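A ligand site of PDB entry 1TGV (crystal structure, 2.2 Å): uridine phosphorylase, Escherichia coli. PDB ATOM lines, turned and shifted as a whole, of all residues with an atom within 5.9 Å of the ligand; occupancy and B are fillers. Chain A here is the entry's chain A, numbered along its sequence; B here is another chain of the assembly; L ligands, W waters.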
ATOM      1  N   GLY A  29      12.786 -18.326  13.004  1.00  0.00           N
ATOM      2  CA  GLY A  29      13.250 -19.492  13.743  1.00  0.00           C
ATOM      3  C   GLY A  29      14.738 -19.709  13.609  1.00  0.00           C
ATOM      4  O   GLY A  29      15.391 -20.129  14.570  1.00  0.00           O
ATOM      5  N   GLY A  71      14.955 -20.202  17.423  1.00  0.00           N
ATOM      6  CA  GLY A  71      15.480 -21.552  17.365  1.00  0.00           C
ATOM      7  C   GLY A  71      14.282 -22.407  17.002  1.00  0.00           C
ATOM      8  O   GLY A  71      13.158 -21.893  16.947  1.00  0.00           O
ATOM      9  N   ILE A  72      14.491 -23.698  16.754  1.00  0.00           N
ATOM     10  CA  ILE A  72      13.366 -24.565  16.385  1.00  0.00           C
ATOM     11  C   ILE A  72      12.598 -25.073  17.604  1.00  0.00           C
ATOM     12  O   ILE A  72      13.206 -25.535  18.572  1.00  0.00           O
ATOM     13  CB  ILE A  72      13.855 -25.802  15.583  1.00  0.00           C
ATOM     14  CG1 ILE A  72      14.414 -25.371  14.229  1.00  0.00           C
ATOM     15  CG2 ILE A  72      12.695 -26.775  15.397  1.00  0.00           C
ATOM     16  CD1 ILE A  72      15.117 -26.492  13.474  1.00  0.00           C
ATOM     17  N   GLY A  73      11.280 -24.978  17.575  1.00  0.00           N
ATOM     18  CA  GLY A  73      10.477 -25.494  18.667  1.00  0.00           C
ATOM     19  C   GLY A  73       9.928 -24.511  19.693  1.00  0.00           C
ATOM     20  O   GLY A  73      10.506 -23.453  19.958  1.00  0.00           O
ATOM     21  N   ARG A  94       6.083 -13.627  13.698  1.00  0.00           N
ATOM     22  CA  ARG A  94       6.931 -14.738  13.309  1.00  0.00           C
ATOM     23  C   ARG A  94       6.929 -14.950  11.805  1.00  0.00           C
ATOM     24  O   ARG A  94       5.876 -14.958  11.159  1.00  0.00           O
ATOM     25  CB  ARG A  94       6.500 -16.030  13.989  1.00  0.00           C
ATOM     26  CG  ARG A  94       7.160 -17.282  13.399  1.00  0.00           C
ATOM     27  CD  ARG A  94       6.872 -18.545  14.201  1.00  0.00           C
ATOM     28  NE  ARG A  94       6.891 -19.738  13.345  1.00  0.00           N
ATOM     29  CZ  ARG A  94       7.952 -20.143  12.660  1.00  0.00           C
ATOM     30  NH1 ARG A  94       9.098 -19.469  12.736  1.00  0.00           N
ATOM     31  NH2 ARG A  94       7.855 -21.192  11.854  1.00  0.00           N
ATOM     32  N   GLY A  96       8.433 -17.713   9.172  1.00  0.00           N
ATOM     33  CA  GLY A  96       9.108 -18.998   9.089  1.00  0.00           C
ATOM     34  C   GLY A  96       9.043 -19.658   7.724  1.00  0.00           C
ATOM     35  O   GLY A  96       8.721 -19.037   6.699  1.00  0.00           O
ATOM     36  N   THR A  97       9.393 -20.945   7.724  1.00  0.00           N
ATOM     37  CA  THR A  97       9.382 -21.777   6.524  1.00  0.00           C
ATOM     38  C   THR A  97       8.361 -22.857   6.857  1.00  0.00           C
ATOM     39  O   THR A  97       8.172 -23.188   8.023  1.00  0.00           O
ATOM     40  CB  THR A  97      10.758 -22.397   6.269  1.00  0.00           C
ATOM     41  OG1 THR A  97      11.209 -23.090   7.436  1.00  0.00           O
ATOM     42  CG2 THR A  97      11.763 -21.293   5.921  1.00  0.00           C
ATOM     43  N   THR A  98       7.692 -23.395   5.849  1.00  0.00           N
ATOM     44  CA  THR A  98       6.675 -24.400   6.130  1.00  0.00           C
ATOM     45  C   THR A  98       6.436 -25.414   5.024  1.00  0.00           C
ATOM     46  O   THR A  98       6.825 -25.207   3.865  1.00  0.00           O
ATOM     47  CB  THR A  98       5.324 -23.743   6.467  1.00  0.00           C
ATOM     48  OG1 THR A  98       4.364 -24.750   6.797  1.00  0.00           O
ATOM     49  CG2 THR A  98       4.804 -22.931   5.281  1.00  0.00           C
ATOM     50  N   GLY A  99       5.799 -26.517   5.398  1.00  0.00           N
ATOM     51  CA  GLY A  99       5.461 -27.558   4.448  1.00  0.00           C
ATOM     52  C   GLY A  99       3.956 -27.581   4.250  1.00  0.00           C
ATOM     53  O   GLY A  99       3.202 -27.761   5.207  1.00  0.00           O
ATOM     54  N   ALA A 100       3.511 -27.361   3.020  1.00  0.00           N
ATOM     55  CA  ALA A 100       2.082 -27.358   2.729  1.00  0.00           C
ATOM     56  C   ALA A 100       1.565 -28.776   2.637  1.00  0.00           C
ATOM     57  O   ALA A 100       2.292 -29.688   2.236  1.00  0.00           O
ATOM     58  CB  ALA A 100       1.820 -26.609   1.421  1.00  0.00           C
ATOM     59  N   THR A 164       7.677 -31.960  16.666  1.00  0.00           N
ATOM     60  CA  THR A 164       8.669 -32.744  15.915  1.00  0.00           C
ATOM     61  C   THR A 164       8.576 -32.504  14.419  1.00  0.00           C
ATOM     62  O   THR A 164       7.494 -32.210  13.883  1.00  0.00           O
ATOM     63  CB  THR A 164       8.519 -34.262  16.137  1.00  0.00           C
ATOM     64  OG1 THR A 164       7.230 -34.688  15.675  1.00  0.00           O
ATOM     65  CG2 THR A 164       8.685 -34.618  17.602  1.00  0.00           C
ATOM     66  N   PHE A 165       9.701 -32.628  13.745  1.00  0.00           N
ATOM     67  CA  PHE A 165       9.775 -32.446  12.308  1.00  0.00           C
ATOM     68  C   PHE A 165       9.336 -33.727  11.598  1.00  0.00           C
ATOM     69  O   PHE A 165       8.780 -33.679  10.512  1.00  0.00           O
ATOM     70  CB  PHE A 165      11.201 -32.100  11.886  1.00  0.00           C
ATOM     71  CG  PHE A 165      11.344 -31.774  10.421  1.00  0.00           C
ATOM     72  CD1 PHE A 165      11.030 -30.517   9.931  1.00  0.00           C
ATOM     73  CD2 PHE A 165      11.787 -32.752   9.527  1.00  0.00           C
ATOM     74  CE1 PHE A 165      11.147 -30.220   8.559  1.00  0.00           C
ATOM     75  CE2 PHE A 165      11.907 -32.477   8.158  1.00  0.00           C
ATOM     76  CZ  PHE A 165      11.582 -31.207   7.672  1.00  0.00           C
ATOM     77  N   GLN A 169       4.730 -34.894  12.027  1.00  0.00           N
ATOM     78  CA  GLN A 169       4.311 -34.421  10.707  1.00  0.00           C
ATOM     79  C   GLN A 169       4.181 -35.668   9.819  1.00  0.00           C
ATOM     80  O   GLN A 169       4.213 -35.595   8.579  1.00  0.00           O
ATOM     81  CB  GLN A 169       5.336 -33.439  10.138  1.00  0.00           C
ATOM     82  CG  GLN A 169       5.422 -32.148  10.960  1.00  0.00           C
ATOM     83  CD  GLN A 169       6.415 -31.142  10.400  1.00  0.00           C
ATOM     84  OE1 GLN A 169       6.413 -30.863   9.202  1.00  0.00           O
ATOM     85  NE2 GLN A 169       7.234 -30.572  11.261  1.00  0.00           N
ATOM     86  N   ARG A 171       6.134 -38.207   8.961  1.00  0.00           N
ATOM     87  CA  ARG A 171       7.151 -38.504   7.960  1.00  0.00           C
ATOM     88  C   ARG A 171       7.622 -39.930   8.295  1.00  0.00           C
ATOM     89  O   ARG A 171       7.838 -40.243   9.463  1.00  0.00           O
ATOM     90  CB  ARG A 171       8.336 -37.545   8.082  1.00  0.00           C
ATOM     91  CG  ARG A 171       8.177 -36.200   7.382  1.00  0.00           C
ATOM     92  CD  ARG A 171       9.539 -35.497   7.251  1.00  0.00           C
ATOM     93  NE  ARG A 171       9.494 -34.358   6.337  1.00  0.00           N
ATOM     94  CZ  ARG A 171       8.942 -33.182   6.636  1.00  0.00           C
ATOM     95  NH1 ARG A 171       8.377 -32.985   7.814  1.00  0.00           N
ATOM     96  NH2 ARG A 171       8.940 -32.200   5.732  1.00  0.00           N
ATOM     97  N   TYR A 198       2.294 -27.423   7.985  1.00  0.00           N
ATOM     98  CA  TYR A 198       3.022 -27.904   9.156  1.00  0.00           C
ATOM     99  C   TYR A 198       4.202 -26.968   9.391  1.00  0.00           C
ATOM    100  O   TYR A 198       4.922 -26.594   8.460  1.00  0.00           O
ATOM    101  CB  TYR A 198       3.640 -29.287   8.912  1.00  0.00           C
ATOM    102  CG  TYR A 198       2.768 -30.487   9.165  1.00  0.00           C
ATOM    103  CD1 TYR A 198       2.645 -31.479   8.199  1.00  0.00           C
ATOM    104  CD2 TYR A 198       2.107 -30.664  10.384  1.00  0.00           C
ATOM    105  CE1 TYR A 198       1.906 -32.630   8.427  1.00  0.00           C
ATOM    106  CE2 TYR A 198       1.360 -31.813  10.635  1.00  0.00           C
ATOM    107  CZ  TYR A 198       1.263 -32.790   9.646  1.00  0.00           C
ATOM    108  OH  TYR A 198       0.542 -33.931   9.866  1.00  0.00           O
ATOM    109  N   GLU A 199       4.418 -26.603  10.652  1.00  0.00           N
ATOM    110  CA  GLU A 199       5.551 -25.782  11.040  1.00  0.00           C
ATOM    111  C   GLU A 199       5.746 -26.109  12.520  1.00  0.00           C
ATOM    112  O   GLU A 199       4.988 -26.917  13.060  1.00  0.00           O
ATOM    113  CB  GLU A 199       5.312 -24.301  10.746  1.00  0.00           C
ATOM    114  CG  GLU A 199       4.116 -23.680  11.395  1.00  0.00           C
ATOM    115  CD  GLU A 199       4.413 -23.257  12.807  1.00  0.00           C
ATOM    116  OE1 GLU A 199       3.715 -23.739  13.716  1.00  0.00           O
ATOM    117  OE2 GLU A 199       5.352 -22.455  12.995  1.00  0.00           O
ATOM    118  N   MET A 200       6.743 -25.524  13.184  1.00  0.00           N
ATOM    119  CA  MET A 200       7.014 -25.908  14.556  1.00  0.00           C
ATOM    120  C   MET A 200       7.083 -24.884  15.695  1.00  0.00           C
ATOM    121  O   MET A 200       7.650 -25.199  16.746  1.00  0.00           O
ATOM    122  CB  MET A 200       8.308 -26.728  14.574  1.00  0.00           C
ATOM    123  CG  MET A 200       8.259 -27.967  13.691  1.00  0.00           C
ATOM    124  SD  MET A 200       9.848 -28.809  13.510  1.00  0.00           S
ATOM    125  CE  MET A 200      10.034 -29.632  15.113  1.00  0.00           C
ATOM    126  N   GLU A 201       6.522 -23.696  15.526  1.00  0.00           N
ATOM    127  CA  GLU A 201       6.580 -22.713  16.609  1.00  0.00           C
ATOM    128  C   GLU A 201       5.308 -21.916  16.837  1.00  0.00           C
ATOM    129  O   GLU A 201       5.133 -21.326  17.905  1.00  0.00           O
ATOM    130  CB  GLU A 201       7.725 -21.710  16.375  1.00  0.00           C
ATOM    131  CG  GLU A 201       9.149 -22.250  16.439  1.00  0.00           C
ATOM    132  CD  GLU A 201       9.549 -23.016  15.183  1.00  0.00           C
ATOM    133  OE1 GLU A 201       9.182 -22.580  14.081  1.00  0.00           O
ATOM    134  OE2 GLU A 201      10.254 -24.041  15.309  1.00  0.00           O
ATOM    135  N   ILE A 223       8.172 -23.994   1.345  1.00  0.00           N
ATOM    136  CA  ILE A 223       9.385 -24.500   0.713  1.00  0.00           C
ATOM    137  C   ILE A 223       9.189 -25.943   0.229  1.00  0.00           C
ATOM    138  O   ILE A 223      10.064 -26.516  -0.409  1.00  0.00           O
ATOM    139  CB  ILE A 223      10.603 -24.455   1.668  1.00  0.00           C
ATOM    140  CG1 ILE A 223      10.334 -25.322   2.902  1.00  0.00           C
ATOM    141  CG2 ILE A 223      10.888 -23.012   2.053  1.00  0.00           C
ATOM    142  CD1 ILE A 223      11.522 -25.432   3.855  1.00  0.00           C
ATOM    143  N   VAL A 224       8.034 -26.513   0.542  1.00  0.00           N
ATOM    144  CA  VAL A 224       7.731 -27.863   0.119  1.00  0.00           C
ATOM    145  C   VAL A 224       6.261 -28.169   0.308  1.00  0.00           C
ATOM    146  O   VAL A 224       5.616 -27.586   1.176  1.00  0.00           O
ATOM    147  CB  VAL A 224       8.572 -28.909   0.911  1.00  0.00           C
ATOM    148  CG1 VAL A 224       8.151 -28.918   2.372  1.00  0.00           C
ATOM    149  CG2 VAL A 224       8.400 -30.285   0.283  1.00  0.00           C
ATOM    150  N   ARG A 226       3.868 -31.427   0.850  1.00  0.00           N
ATOM    151  CA  ARG A 226       3.795 -32.849   1.150  1.00  0.00           C
ATOM    152  C   ARG A 226       2.938 -33.679   0.190  1.00  0.00           C
ATOM    153  O   ARG A 226       3.150 -34.885   0.065  1.00  0.00           O
ATOM    154  CB  ARG A 226       3.304 -33.041   2.581  1.00  0.00           C
ATOM    155  CG  ARG A 226       4.173 -32.366   3.634  1.00  0.00           C
ATOM    156  CD  ARG A 226       5.535 -33.032   3.714  1.00  0.00           C
ATOM    157  NE  ARG A 226       5.392 -34.434   4.122  1.00  0.00           N
ATOM    158  CZ  ARG A 226       5.118 -34.817   5.364  1.00  0.00           C
ATOM    159  NH1 ARG A 226       4.947 -33.908   6.322  1.00  0.00           N
ATOM    160  NH2 ARG A 226       4.974 -36.107   5.647  1.00  0.00           N
ATOM    161  N   PHE B  10      18.463 -33.266   6.410  1.00  0.00           N
ATOM    162  CA  PHE B  10      17.876 -31.950   6.166  1.00  0.00           C
ATOM    163  C   PHE B  10      18.409 -30.793   7.007  1.00  0.00           C
ATOM    164  O   PHE B  10      18.528 -29.673   6.502  1.00  0.00           O
ATOM    165  CB  PHE B  10      16.356 -31.995   6.323  1.00  0.00           C
ATOM    166  CG  PHE B  10      15.680 -30.717   5.889  1.00  0.00           C
ATOM    167  CD1 PHE B  10      15.298 -30.528   4.556  1.00  0.00           C
ATOM    168  CD2 PHE B  10      15.474 -29.679   6.795  1.00  0.00           C
ATOM    169  CE1 PHE B  10      14.746 -29.320   4.143  1.00  0.00           C
ATOM    170  CE2 PHE B  10      14.920 -28.463   6.376  1.00  0.00           C
ATOM    171  CZ  PHE B  10      14.562 -28.287   5.052  1.00  0.00           C
ATOM    172  N   HIS B  11      18.737 -31.027   8.275  1.00  0.00           N
ATOM    173  CA  HIS B  11      19.204 -29.912   9.110  1.00  0.00           C
ATOM    174  C   HIS B  11      20.680 -29.872   9.504  1.00  0.00           C
ATOM    175  O   HIS B  11      21.308 -28.814   9.428  1.00  0.00           O
ATOM    176  CB  HIS B  11      18.376 -29.840  10.406  1.00  0.00           C
ATOM    177  CG  HIS B  11      16.895 -29.768  10.179  1.00  0.00           C
ATOM    178  ND1 HIS B  11      16.121 -30.884   9.910  1.00  0.00           N
ATOM    179  CD2 HIS B  11      16.042 -28.718  10.209  1.00  0.00           C
ATOM    180  CE1 HIS B  11      14.856 -30.519   9.791  1.00  0.00           C
ATOM    181  NE2 HIS B  11      14.779 -29.213   9.964  1.00  0.00           N
ATOM    182  N   ARG B  51      21.852 -23.388  12.094  1.00  0.00           N
ATOM    183  CA  ARG B  51      20.820 -23.136  13.089  1.00  0.00           C
ATOM    184  C   ARG B  51      21.482 -23.415  14.452  1.00  0.00           C
ATOM    185  O   ARG B  51      22.634 -23.034  14.657  1.00  0.00           O
ATOM    186  CB  ARG B  51      19.618 -24.061  12.860  1.00  0.00           C
ATOM    187  CG  ARG B  51      18.744 -23.643  11.662  1.00  0.00           C
ATOM    188  CD  ARG B  51      17.578 -24.608  11.434  1.00  0.00           C
ATOM    189  NE  ARG B  51      16.686 -24.161  10.375  1.00  0.00           N
ATOM    190  CZ  ARG B  51      15.648 -23.346  10.536  1.00  0.00           C
ATOM    191  NH1 ARG B  51      15.333 -22.878  11.740  1.00  0.00           N
ATOM    192  NH2 ARG B  51      14.904 -23.007   9.486  1.00  0.00           N
ATOM    193  N   ILE B  79      15.134 -33.595  16.275  1.00  0.00           N
ATOM    194  CA  ILE B  79      15.661 -33.451  14.924  1.00  0.00           C
ATOM    195  C   ILE B  79      17.108 -33.929  14.909  1.00  0.00           C
ATOM    196  O   ILE B  79      17.482 -34.778  14.099  1.00  0.00           O
ATOM    197  CB  ILE B  79      15.596 -31.983  14.464  1.00  0.00           C
ATOM    198  CG1 ILE B  79      14.153 -31.618  14.131  1.00  0.00           C
ATOM    199  CG2 ILE B  79      16.530 -31.760  13.279  1.00  0.00           C
ATOM    200  CD1 ILE B  79      13.962 -30.176  13.693  1.00  0.00           C
HETATM  201  F1  LIG L   1       9.246 -27.377   5.094  1.00  0.00           F
HETATM  202  C1  LIG L   1       8.976 -27.500   6.411  1.00  0.00           C
HETATM  203  C2  LIG L   1       8.287 -28.632   6.904  1.00  0.00           C
HETATM  204  O1  LIG L   1       7.919 -29.523   6.130  1.00  0.00           O
HETATM  205  N1  LIG L   1       8.014 -28.747   8.288  1.00  0.00           N
HETATM  206  C3  LIG L   1       8.416 -27.750   9.207  1.00  0.00           C
HETATM  207  O2  LIG L   1       8.145 -27.912  10.393  1.00  0.00           O
HETATM  208  C4  LIG L   1       9.386 -26.500   7.315  1.00  0.00           C
HETATM  209  N2  LIG L   1       9.121 -26.588   8.717  1.00  0.00           N
HETATM  210  C5  LIG L   1       9.621 -25.413   9.559  1.00  0.00           C
HETATM  211  C6  LIG L   1       9.375 -25.433  11.108  1.00  0.00           C
HETATM  212  O3  LIG L   1       8.795 -24.179  11.513  1.00  0.00           O
HETATM  213  C7  LIG L   1      10.756 -25.658  11.759  1.00  0.00           C
HETATM  214  O4  LIG L   1      11.124 -24.518  12.556  1.00  0.00           O
HETATM  215  C8  LIG L   1      11.717 -25.756  10.599  1.00  0.00           C
HETATM  216  O5  LIG L   1      11.063 -25.223   9.426  1.00  0.00           O
HETATM  217  C9  LIG L   1      12.277 -27.174  10.429  1.00  0.00           C
HETATM  218  O6  LIG L   1      13.185 -27.203   9.332  1.00  0.00           O
HETATM  219  O   HOH W   1       5.706 -31.372   6.659  1.00  0.00           O
HETATM  220  O   HOH W   2      12.887 -25.476   7.414  1.00  0.00           O
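The guanidinium group of Arg 94 is in hydrogen-bond range of an oxygen (O3) of the ligand.
N1 of the ligand is in hydrogen-bond range of OE1 of Gln 169, at 2.8 Å.
The side-chain hydroxyl (OG1) of Thr 97 sits at hydrogen-bond distance from an oxygen (O5) of the ligand (2.9 Å).
The guanidinium group of Arg 171 sits at hydrogen-bond distance from an oxygen (O1) of the ligand (2.9 Å).
N of Met 200 sits at hydrogen-bond distance from O3 of the ligand (3.0 Å).
A ring nitrogen (NE2) of His 11 of chain B lies within hydrogen-bond range of an oxygen (O6) of the ligand.
OE2 of Glu 201 sits at hydrogen-bond distance from O4 of the ligand, 2.9 Å away.
The backbone carbonyl oxygen (O) of Tyr 198 lies within hydrogen-bond range of the side-chain hydroxyl (OG1) of Thr 98, at 2.5 Å.
O of Gln 169 lies within hydrogen-bond range of NH1 of Arg 226 (2.9 Å).
O of Gly 99 sits at hydrogen-bond distance from N of Tyr 198 (2.9 Å).
O of Val 224 is in hydrogen-bond range of N of Ala 100.
OE2 of Glu 199 sits at hydrogen-bond distance from N of Glu 201 (3.1 Å).
The side-chain carboxylate (OE1) of Glu 201 lies within salt-bridge range of the guanidinium group (NH2) of Arg 94 (2.9 Å).
OE2 of Glu 201 sits at hydrogen-bond distance from N of Gly 73.
The guanidinium group (NH2) of Arg 94 lies within salt-bridge range of the side-chain carboxylate (OE2) of Glu 199 (3.0 Å).
F1 of the ligand lies close to O of Thr 98, at 3.5 Å.
Residues that only touch the ligand: Ile 72, Gly 99, Phe 165, Tyr 198, Glu 199, Ile 223, Val 224 and Phe 10 of chain B.
Hydrophobic or aromatic side chains within 4 Å of the ligand: Ile 72, Phe 165, Met 200, Ile 223, Val 224, Phe 10 of chain B and His 11 of chain B.
16 residues have an atom within 4 Å of the ligand: Ile 72, Arg 94, Thr 97, Thr 98, Gly 99, Phe 165, Gln 169, Arg 171, Tyr 198, Glu 199, Met 200, Glu 201, Ile 223, Val 224, Phe 10 of chain B and His 11 of chain B.
Water W2 lies within hydrogen-bond range of an oxygen (O6) of the ligand and the side-chain hydroxyl (OG1) of Thr 97.
Water W1 lies within hydrogen-bond range of NH1 of Arg 226 (2.7 Å), OE1 of Gln 169 (2.7 Å), O1 of the ligand (2.9 Å) and NH1 of Arg 171 (3.3 Å).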
